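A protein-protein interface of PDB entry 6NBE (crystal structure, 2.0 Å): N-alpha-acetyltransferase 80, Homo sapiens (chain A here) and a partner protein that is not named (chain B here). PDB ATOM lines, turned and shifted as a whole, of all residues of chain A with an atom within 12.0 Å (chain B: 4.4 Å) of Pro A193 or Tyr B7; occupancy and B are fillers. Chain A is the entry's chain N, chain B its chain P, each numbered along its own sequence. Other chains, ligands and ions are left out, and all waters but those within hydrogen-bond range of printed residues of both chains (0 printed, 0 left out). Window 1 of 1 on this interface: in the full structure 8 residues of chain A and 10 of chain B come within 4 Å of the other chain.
The backbone carbonyl oxygen (O) of Pro A194 is in hydrogen-bond range of the side-chain hydroxyl (OH) of Tyr B7, at 2.8 Å.
O of Pro A195 sits at hydrogen-bond distance from NE2 of His B134, 2.9 Å away.
O of Pro A191 is in hydrogen-bond range of NE1 of Trp B4 (2.8 Å).
The backbone carbonyl oxygen (O) of Pro A195 lies within hydrogen-bond range of the side-chain hydroxyl (OH) of Tyr B7.
A ring nitrogen (NE2) of His B134 is in hydrogen-bond range of the side-chain hydroxyl of Tyr B7, 3.0 Å away.
Gly B3 touches Pro A193.
Trp B4 touches Pro A193 (CZ2 to CA, 3.6 Å).
Pro A193 touches Tyr B7 (CB to CE1, 3.8 Å).
Pro A194 touches Trp B4 (CD to CH2, 3.9 Å).
CG of Pro A194 touches CD2 of Leu B135, 3.9 Å away.
CD1 of Leu A196 touches O of Ala B6, 3.8 Å away.
CD2 of Leu A196 touches CE2 of Tyr B7, 3.3 Å away.
Leu A196 touches Asn B10 (CD1 to OD1, 3.9 Å).
Leu A196 touches His B134 (CA to NE2, 3.5 Å).
N of Pro A197 touches CE1 of His B134, at 3.4 Å.
Printed residues of chain B within 4 Å of Leu A190: Trp B4 (3.6 Å).
Of the printed residues of chain B, Pro A191 touches Trp B4.
Pro A192 touches none of the printed residues of chain B.
Pro A193 touches three residues of chain B.
Printed residues of chain B within 4 Å of Pro A194: Trp B4 (3.9 Å), Tyr B7 (2.8 Å) and Leu B135 (3.9 Å).
Of the printed residues of chain B, Pro A195 touches Tyr B7 and His B134.
Printed residues of chain B within 4 Å of Pro A197: His B134 (3.4 Å).
Cys A199 touches none of the printed residues of chain B.
Of chain A, only Pro A193 (3.5 Å) comes within 4 Å of Gly B3.
Trp B4 touches four residues of chain A.
No residue of chain A comes within 4 Å of Asn B5.
Ala B6 touches just one residue of chain A: Leu A196 (3.8 Å).
Tyr B7 touches just these residues of chain A: Pro A193, Pro A194, Pro A195 and Leu A196.
No residue of chain A comes within 4 Å of Ile B8.
No residue of chain A comes within 4 Å of Asp B9.
Asn B10 touches just one residue of chain A: Leu A196 (3.9 Å).
No residue of chain A comes within 4 Å of Met B131.
Of the printed residues of chain A, His B134 touches Pro A195 (2.9 Å), Leu A196 (3.5 Å) and Pro A197 (3.4 Å).
Leu B135 touches just one residue of chain A: Pro A194 (3.9 Å).
The nearest printed residue of chain B that does not touch Pro A193 is Leu B135 (6.2 Å).
The nearest printed residue of chain B that does not touch Pro A191 is Gly B3 (7.4 Å).
Of the 10 printed residues of chain A, 7 touch a printed residue of chain B.
Printed residues of chain A that touch a printed residue of chain B: Leu A190, Pro A191, Pro A193, Pro A194, Pro A195, Leu A196 and Pro A197.
Hydrophobic or aromatic side chains of chain A that line the printed part of chain B: Leu A190, Pro A193, Pro A194, Leu A196 and Pro A197.
Hydrophobic or aromatic side chains of chain B within 4 Å of the printed part of chain A: Trp B4, Tyr B7, His B134 and Leu B135.
Among the printed residues, 15 pairs touch across the chains.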
ATOM      1  N   LEU A 190      13.063   7.588 -14.348  1.00  0.00           N
ATOM      2  CA  LEU A 190      14.266   6.821 -14.681  1.00  0.00           C
ATOM      3  C   LEU A 190      15.470   7.431 -13.964  1.00  0.00           C
ATOM      4  O   LEU A 190      16.052   8.404 -14.443  1.00  0.00           O
ATOM      5  CB  LEU A 190      14.485   6.804 -16.193  1.00  0.00           C
ATOM      6  CG  LEU A 190      14.865   5.458 -16.809  1.00  0.00           C
ATOM      7  CD1 LEU A 190      14.064   5.209 -18.086  1.00  0.00           C
ATOM      8  CD2 LEU A 190      16.354   5.399 -17.102  1.00  0.00           C
ATOM      9  N   PRO A 191      15.848   6.866 -12.819  1.00  0.00           N
ATOM     10  CA  PRO A 191      16.891   7.495 -11.993  1.00  0.00           C
ATOM     11  C   PRO A 191      18.270   7.287 -12.588  1.00  0.00           C
ATOM     12  O   PRO A 191      18.494   6.351 -13.376  1.00  0.00           O
ATOM     13  CB  PRO A 191      16.753   6.784 -10.634  1.00  0.00           C
ATOM     14  CG  PRO A 191      16.193   5.446 -10.975  1.00  0.00           C
ATOM     15  CD  PRO A 191      15.276   5.672 -12.170  1.00  0.00           C
ATOM     16  N   PRO A 192      19.223   8.143 -12.228  1.00  0.00           N
ATOM     17  CA  PRO A 192      20.579   8.053 -12.795  1.00  0.00           C
ATOM     18  C   PRO A 192      21.325   6.843 -12.265  1.00  0.00           C
ATOM     19  O   PRO A 192      21.178   6.473 -11.090  1.00  0.00           O
ATOM     20  CB  PRO A 192      21.242   9.358 -12.321  1.00  0.00           C
ATOM     21  CG  PRO A 192      20.519   9.673 -11.019  1.00  0.00           C
ATOM     22  CD  PRO A 192      19.082   9.297 -11.316  1.00  0.00           C
ATOM     23  N   PRO A 193      22.156   6.212 -13.091  1.00  0.00           N
ATOM     24  CA  PRO A 193      22.957   5.073 -12.613  1.00  0.00           C
ATOM     25  C   PRO A 193      24.038   5.526 -11.650  1.00  0.00           C
ATOM     26  O   PRO A 193      24.670   6.576 -11.860  1.00  0.00           O
ATOM     27  CB  PRO A 193      23.567   4.502 -13.905  1.00  0.00           C
ATOM     28  CG  PRO A 193      23.606   5.678 -14.849  1.00  0.00           C
ATOM     29  CD  PRO A 193      22.346   6.457 -14.535  1.00  0.00           C
ATOM     30  N   PRO A 194      24.292   4.768 -10.585  1.00  0.00           N
ATOM     31  CA  PRO A 194      25.466   5.049  -9.745  1.00  0.00           C
ATOM     32  C   PRO A 194      26.737   4.741 -10.514  1.00  0.00           C
ATOM     33  O   PRO A 194      26.679   4.156 -11.608  1.00  0.00           O
ATOM     34  CB  PRO A 194      25.285   4.098  -8.552  1.00  0.00           C
ATOM     35  CG  PRO A 194      24.531   2.944  -9.124  1.00  0.00           C
ATOM     36  CD  PRO A 194      23.577   3.553 -10.139  1.00  0.00           C
ATOM     37  N   PRO A 195      27.905   5.112  -9.994  1.00  0.00           N
ATOM     38  CA  PRO A 195      29.141   4.856 -10.745  1.00  0.00           C
ATOM     39  C   PRO A 195      29.432   3.365 -10.790  1.00  0.00           C
ATOM     40  O   PRO A 195      29.145   2.620  -9.848  1.00  0.00           O
ATOM     41  CB  PRO A 195      30.218   5.616  -9.957  1.00  0.00           C
ATOM     42  CG  PRO A 195      29.476   6.414  -8.900  1.00  0.00           C
ATOM     43  CD  PRO A 195      28.183   5.676  -8.663  1.00  0.00           C
ATOM     44  N   LEU A 196      30.006   2.935 -11.918  1.00  0.00           N
ATOM     45  CA  LEU A 196      30.293   1.535 -12.134  1.00  0.00           C
ATOM     46  C   LEU A 196      31.498   1.101 -11.299  1.00  0.00           C
ATOM     47  O   LEU A 196      32.235   1.938 -10.770  1.00  0.00           O
ATOM     48  CB  LEU A 196      30.560   1.271 -13.612  1.00  0.00           C
ATOM     49  CG  LEU A 196      29.366   0.844 -14.464  1.00  0.00           C
ATOM     50  CD1 LEU A 196      29.753   0.867 -15.938  1.00  0.00           C
ATOM     51  CD2 LEU A 196      28.883  -0.539 -14.066  1.00  0.00           C
ATOM     52  N   PRO A 197      31.729  -0.206 -11.170  1.00  0.00           N
ATOM     53  CA  PRO A 197      32.917  -0.665 -10.440  1.00  0.00           C
ATOM     54  C   PRO A 197      34.168  -0.156 -11.132  1.00  0.00           C
ATOM     55  O   PRO A 197      34.370  -0.382 -12.330  1.00  0.00           O
ATOM     56  CB  PRO A 197      32.814  -2.198 -10.494  1.00  0.00           C
ATOM     57  CG  PRO A 197      31.397  -2.488 -10.887  1.00  0.00           C
ATOM     58  CD  PRO A 197      30.981  -1.331 -11.760  1.00  0.00           C
ATOM     59  N   GLU A 198      35.018   0.535 -10.371  1.00  0.00           N
ATOM     60  CA  GLU A 198      36.306   0.974 -10.902  1.00  0.00           C
ATOM     61  C   GLU A 198      36.051   1.818 -12.154  1.00  0.00           C
ATOM     62  O   GLU A 198      36.661   1.617 -13.208  1.00  0.00           O
ATOM     63  CB  GLU A 198      37.216  -0.224 -11.192  1.00  0.00           C
ATOM     64  CG  GLU A 198      36.852  -1.495 -10.395  1.00  0.00           C
ATOM     65  CD  GLU A 198      37.924  -1.922  -9.377  1.00  0.00           C
ATOM     66  OE1 GLU A 198      39.019  -2.358  -9.803  1.00  0.00           O
ATOM     67  OE2 GLU A 198      37.659  -1.820  -8.158  1.00  0.00           O
ATOM     68  N   CYS A 199      35.104   2.756 -12.017  1.00  0.00           N
ATOM     69  CA  CYS A 199      34.603   3.650 -13.064  1.00  0.00           C
ATOM     70  C   CYS A 199      33.066   3.530 -13.087  1.00  0.00           C
ATOM     71  O   CYS A 199      32.353   4.451 -13.487  1.00  0.00           O
ATOM     72  CB  CYS A 199      35.144   3.345 -14.449  1.00  0.00           C
ATOM     73  SG  CYS A 199      34.320   4.308 -15.760  1.00  0.00           S
ATOM     74  N   GLY B   3      25.231   6.756 -18.812  1.00  0.00           N
ATOM     75  CA  GLY B   3      23.878   6.254 -18.653  1.00  0.00           C
ATOM     76  C   GLY B   3      23.823   4.799 -18.231  1.00  0.00           C
ATOM     77  O   GLY B   3      24.844   4.194 -17.903  1.00  0.00           O
ATOM     78  N   TRP B   4      22.612   4.240 -18.222  1.00  0.00           N
ATOM     79  CA  TRP B   4      22.460   2.827 -17.895  1.00  0.00           C
ATOM     80  C   TRP B   4      23.052   1.935 -18.977  1.00  0.00           C
ATOM     81  O   TRP B   4      23.443   0.794 -18.696  1.00  0.00           O
ATOM     82  CB  TRP B   4      20.984   2.485 -17.696  1.00  0.00           C
ATOM     83  CG  TRP B   4      20.446   2.962 -16.406  1.00  0.00           C
ATOM     84  CD1 TRP B   4      19.574   3.990 -16.210  1.00  0.00           C
ATOM     85  CD2 TRP B   4      20.743   2.433 -15.112  1.00  0.00           C
ATOM     86  NE1 TRP B   4      19.307   4.134 -14.872  1.00  0.00           N
ATOM     87  CE2 TRP B   4      20.012   3.188 -14.176  1.00  0.00           C
ATOM     88  CE3 TRP B   4      21.555   1.390 -14.655  1.00  0.00           C
ATOM     89  CZ2 TRP B   4      20.071   2.937 -12.805  1.00  0.00           C
ATOM     90  CZ3 TRP B   4      21.614   1.142 -13.294  1.00  0.00           C
ATOM     91  CH2 TRP B   4      20.877   1.915 -12.386  1.00  0.00           C
ATOM     92  N   ASN B   5      23.102   2.424 -20.218  1.00  0.00           N
ATOM     93  CA  ASN B   5      23.690   1.644 -21.299  1.00  0.00           C
ATOM     94  C   ASN B   5      25.164   1.365 -21.060  1.00  0.00           C
ATOM     95  O   ASN B   5      25.686   0.376 -21.590  1.00  0.00           O
ATOM     96  CB  ASN B   5      23.472   2.375 -22.617  1.00  0.00           C
ATOM     97  CG  ASN B   5      22.001   2.585 -22.924  1.00  0.00           C
ATOM     98  OD1 ASN B   5      21.367   1.755 -23.579  1.00  0.00           O
ATOM     99  ND2 ASN B   5      21.442   3.684 -22.430  1.00  0.00           N
ATOM    100  N   ALA B   6      25.836   2.192 -20.255  1.00  0.00           N
ATOM    101  CA  ALA B   6      27.189   1.860 -19.823  1.00  0.00           C
ATOM    102  C   ALA B   6      27.205   0.541 -19.063  1.00  0.00           C
ATOM    103  O   ALA B   6      28.149  -0.249 -19.183  1.00  0.00           O
ATOM    104  CB  ALA B   6      27.755   2.986 -18.953  1.00  0.00           C
ATOM    105  N   TYR B   7      26.166   0.291 -18.264  1.00  0.00           N
ATOM    106  CA  TYR B   7      26.079  -0.977 -17.549  1.00  0.00           C
ATOM    107  C   TYR B   7      25.911  -2.140 -18.511  1.00  0.00           C
ATOM    108  O   TYR B   7      26.451  -3.227 -18.280  1.00  0.00           O
ATOM    109  CB  TYR B   7      24.921  -0.936 -16.562  1.00  0.00           C
ATOM    110  CG  TYR B   7      25.317  -0.330 -15.249  1.00  0.00           C
ATOM    111  CD1 TYR B   7      25.569   1.030 -15.137  1.00  0.00           C
ATOM    112  CD2 TYR B   7      25.460  -1.119 -14.117  1.00  0.00           C
ATOM    113  CE1 TYR B   7      25.944   1.585 -13.938  1.00  0.00           C
ATOM    114  CE2 TYR B   7      25.833  -0.573 -12.916  1.00  0.00           C
ATOM    115  CZ  TYR B   7      26.077   0.781 -12.832  1.00  0.00           C
ATOM    116  OH  TYR B   7      26.450   1.330 -11.628  1.00  0.00           O
ATOM    117  N   ILE B   8      25.170  -1.922 -19.598  1.00  0.00           N
ATOM    118  CA  ILE B   8      24.968  -2.972 -20.587  1.00  0.00           C
ATOM    119  C   ILE B   8      26.276  -3.271 -21.311  1.00  0.00           C
ATOM    120  O   ILE B   8      26.656  -4.435 -21.496  1.00  0.00           O
ATOM    121  CB  ILE B   8      23.853  -2.564 -21.565  1.00  0.00           C
ATOM    122  CG1 ILE B   8      22.596  -2.164 -20.797  1.00  0.00           C
ATOM    123  CG2 ILE B   8      23.564  -3.694 -22.529  1.00  0.00           C
ATOM    124  CD1 ILE B   8      21.891  -3.337 -20.118  1.00  0.00           C
ATOM    125  N   ASP B   9      26.981  -2.219 -21.744  1.00  0.00           N
ATOM    126  CA  ASP B   9      28.303  -2.415 -22.331  1.00  0.00           C
ATOM    127  C   ASP B   9      29.226  -3.145 -21.363  1.00  0.00           C
ATOM    128  O   ASP B   9      29.989  -4.039 -21.757  1.00  0.00           O
ATOM    129  CB  ASP B   9      28.912  -1.067 -22.711  1.00  0.00           C
ATOM    130  CG  ASP B   9      28.099  -0.332 -23.753  1.00  0.00           C
ATOM    131  OD1 ASP B   9      27.489  -1.003 -24.615  1.00  0.00           O
ATOM    132  OD2 ASP B   9      28.073   0.919 -23.714  1.00  0.00           O
ATOM    133  N   ASN B  10      29.152  -2.786 -20.081  1.00  0.00           N
ATOM    134  CA  ASN B  10      29.984  -3.428 -19.071  1.00  0.00           C
ATOM    135  C   ASN B  10      29.675  -4.916 -18.961  1.00  0.00           C
ATOM    136  O   ASN B  10      30.593  -5.745 -18.888  1.00  0.00           O
ATOM    137  CB  ASN B  10      29.765  -2.727 -17.730  1.00  0.00           C
ATOM    138  CG  ASN B  10      30.742  -3.167 -16.672  1.00  0.00           C
ATOM    139  OD1 ASN B  10      31.750  -2.503 -16.434  1.00  0.00           O
ATOM    140  ND2 ASN B  10      30.445  -4.284 -16.018  1.00  0.00           N
ATOM    141  N   LEU B  11      28.392  -5.275 -18.947  1.00  0.00           N
ATOM    142  CA  LEU B  11      28.014  -6.676 -18.826  1.00  0.00           C
ATOM    143  C   LEU B  11      28.357  -7.459 -20.086  1.00  0.00           C
ATOM    144  O   LEU B  11      28.634  -8.662 -20.006  1.00  0.00           O
ATOM    145  CB  LEU B  11      26.517  -6.784 -18.536  1.00  0.00           C
ATOM    146  CG  LEU B  11      26.059  -6.250 -17.178  1.00  0.00           C
ATOM    147  CD1 LEU B  11      24.563  -6.007 -17.161  1.00  0.00           C
ATOM    148  CD2 LEU B  11      26.464  -7.212 -16.059  1.00  0.00           C
ATOM    149  N   MET B 131      27.116  -7.980 -10.437  1.00  0.00           N
ATOM    150  CA  MET B 131      26.532  -6.698 -10.826  1.00  0.00           C
ATOM    151  C   MET B 131      25.428  -6.283  -9.860  1.00  0.00           C
ATOM    152  O   MET B 131      25.308  -5.104  -9.509  1.00  0.00           O
ATOM    153  CB  MET B 131      25.997  -6.767 -12.254  1.00  0.00           C
ATOM    154  CG  MET B 131      25.228  -5.520 -12.692  1.00  0.00           C
ATOM    155  SD  MET B 131      26.236  -4.011 -12.687  1.00  0.00           S
ATOM    156  CE  MET B 131      27.242  -4.275 -14.134  1.00  0.00           C
ATOM    157  N   HIS B 134      26.925  -4.954  -6.758  1.00  0.00           N
ATOM    158  CA  HIS B 134      27.414  -3.603  -6.996  1.00  0.00           C
ATOM    159  C   HIS B 134      26.289  -2.582  -6.898  1.00  0.00           C
ATOM    160  O   HIS B 134      26.459  -1.518  -6.293  1.00  0.00           O
ATOM    161  CB  HIS B 134      28.074  -3.517  -8.366  1.00  0.00           C
ATOM    162  CG  HIS B 134      28.305  -2.116  -8.833  1.00  0.00           C
ATOM    163  ND1 HIS B 134      29.210  -1.272  -8.228  1.00  0.00           N
ATOM    164  CD2 HIS B 134      27.743  -1.408  -9.841  1.00  0.00           C
ATOM    165  CE1 HIS B 134      29.202  -0.105  -8.847  1.00  0.00           C
ATOM    166  NE2 HIS B 134      28.321  -0.161  -9.830  1.00  0.00           N
ATOM    167  N   LEU B 135      25.130  -2.890  -7.482  1.00  0.00           N
ATOM    168  CA  LEU B 135      24.027  -1.935  -7.473  1.00  0.00           C
ATOM    169  C   LEU B 135      23.417  -1.811  -6.085  1.00  0.00           C
ATOM    170  O   LEU B 135      23.083  -0.704  -5.649  1.00  0.00           O
ATOM    171  CB  LEU B 135      22.974  -2.346  -8.499  1.00  0.00           C
ATOM    172  CG  LEU B 135      23.402  -2.103  -9.947  1.00  0.00           C
ATOM    173  CD1 LEU B 135      22.498  -2.830 -10.925  1.00  0.00           C
ATOM    174  CD2 LEU B 135      23.421  -0.604 -10.248  1.00  0.00           C
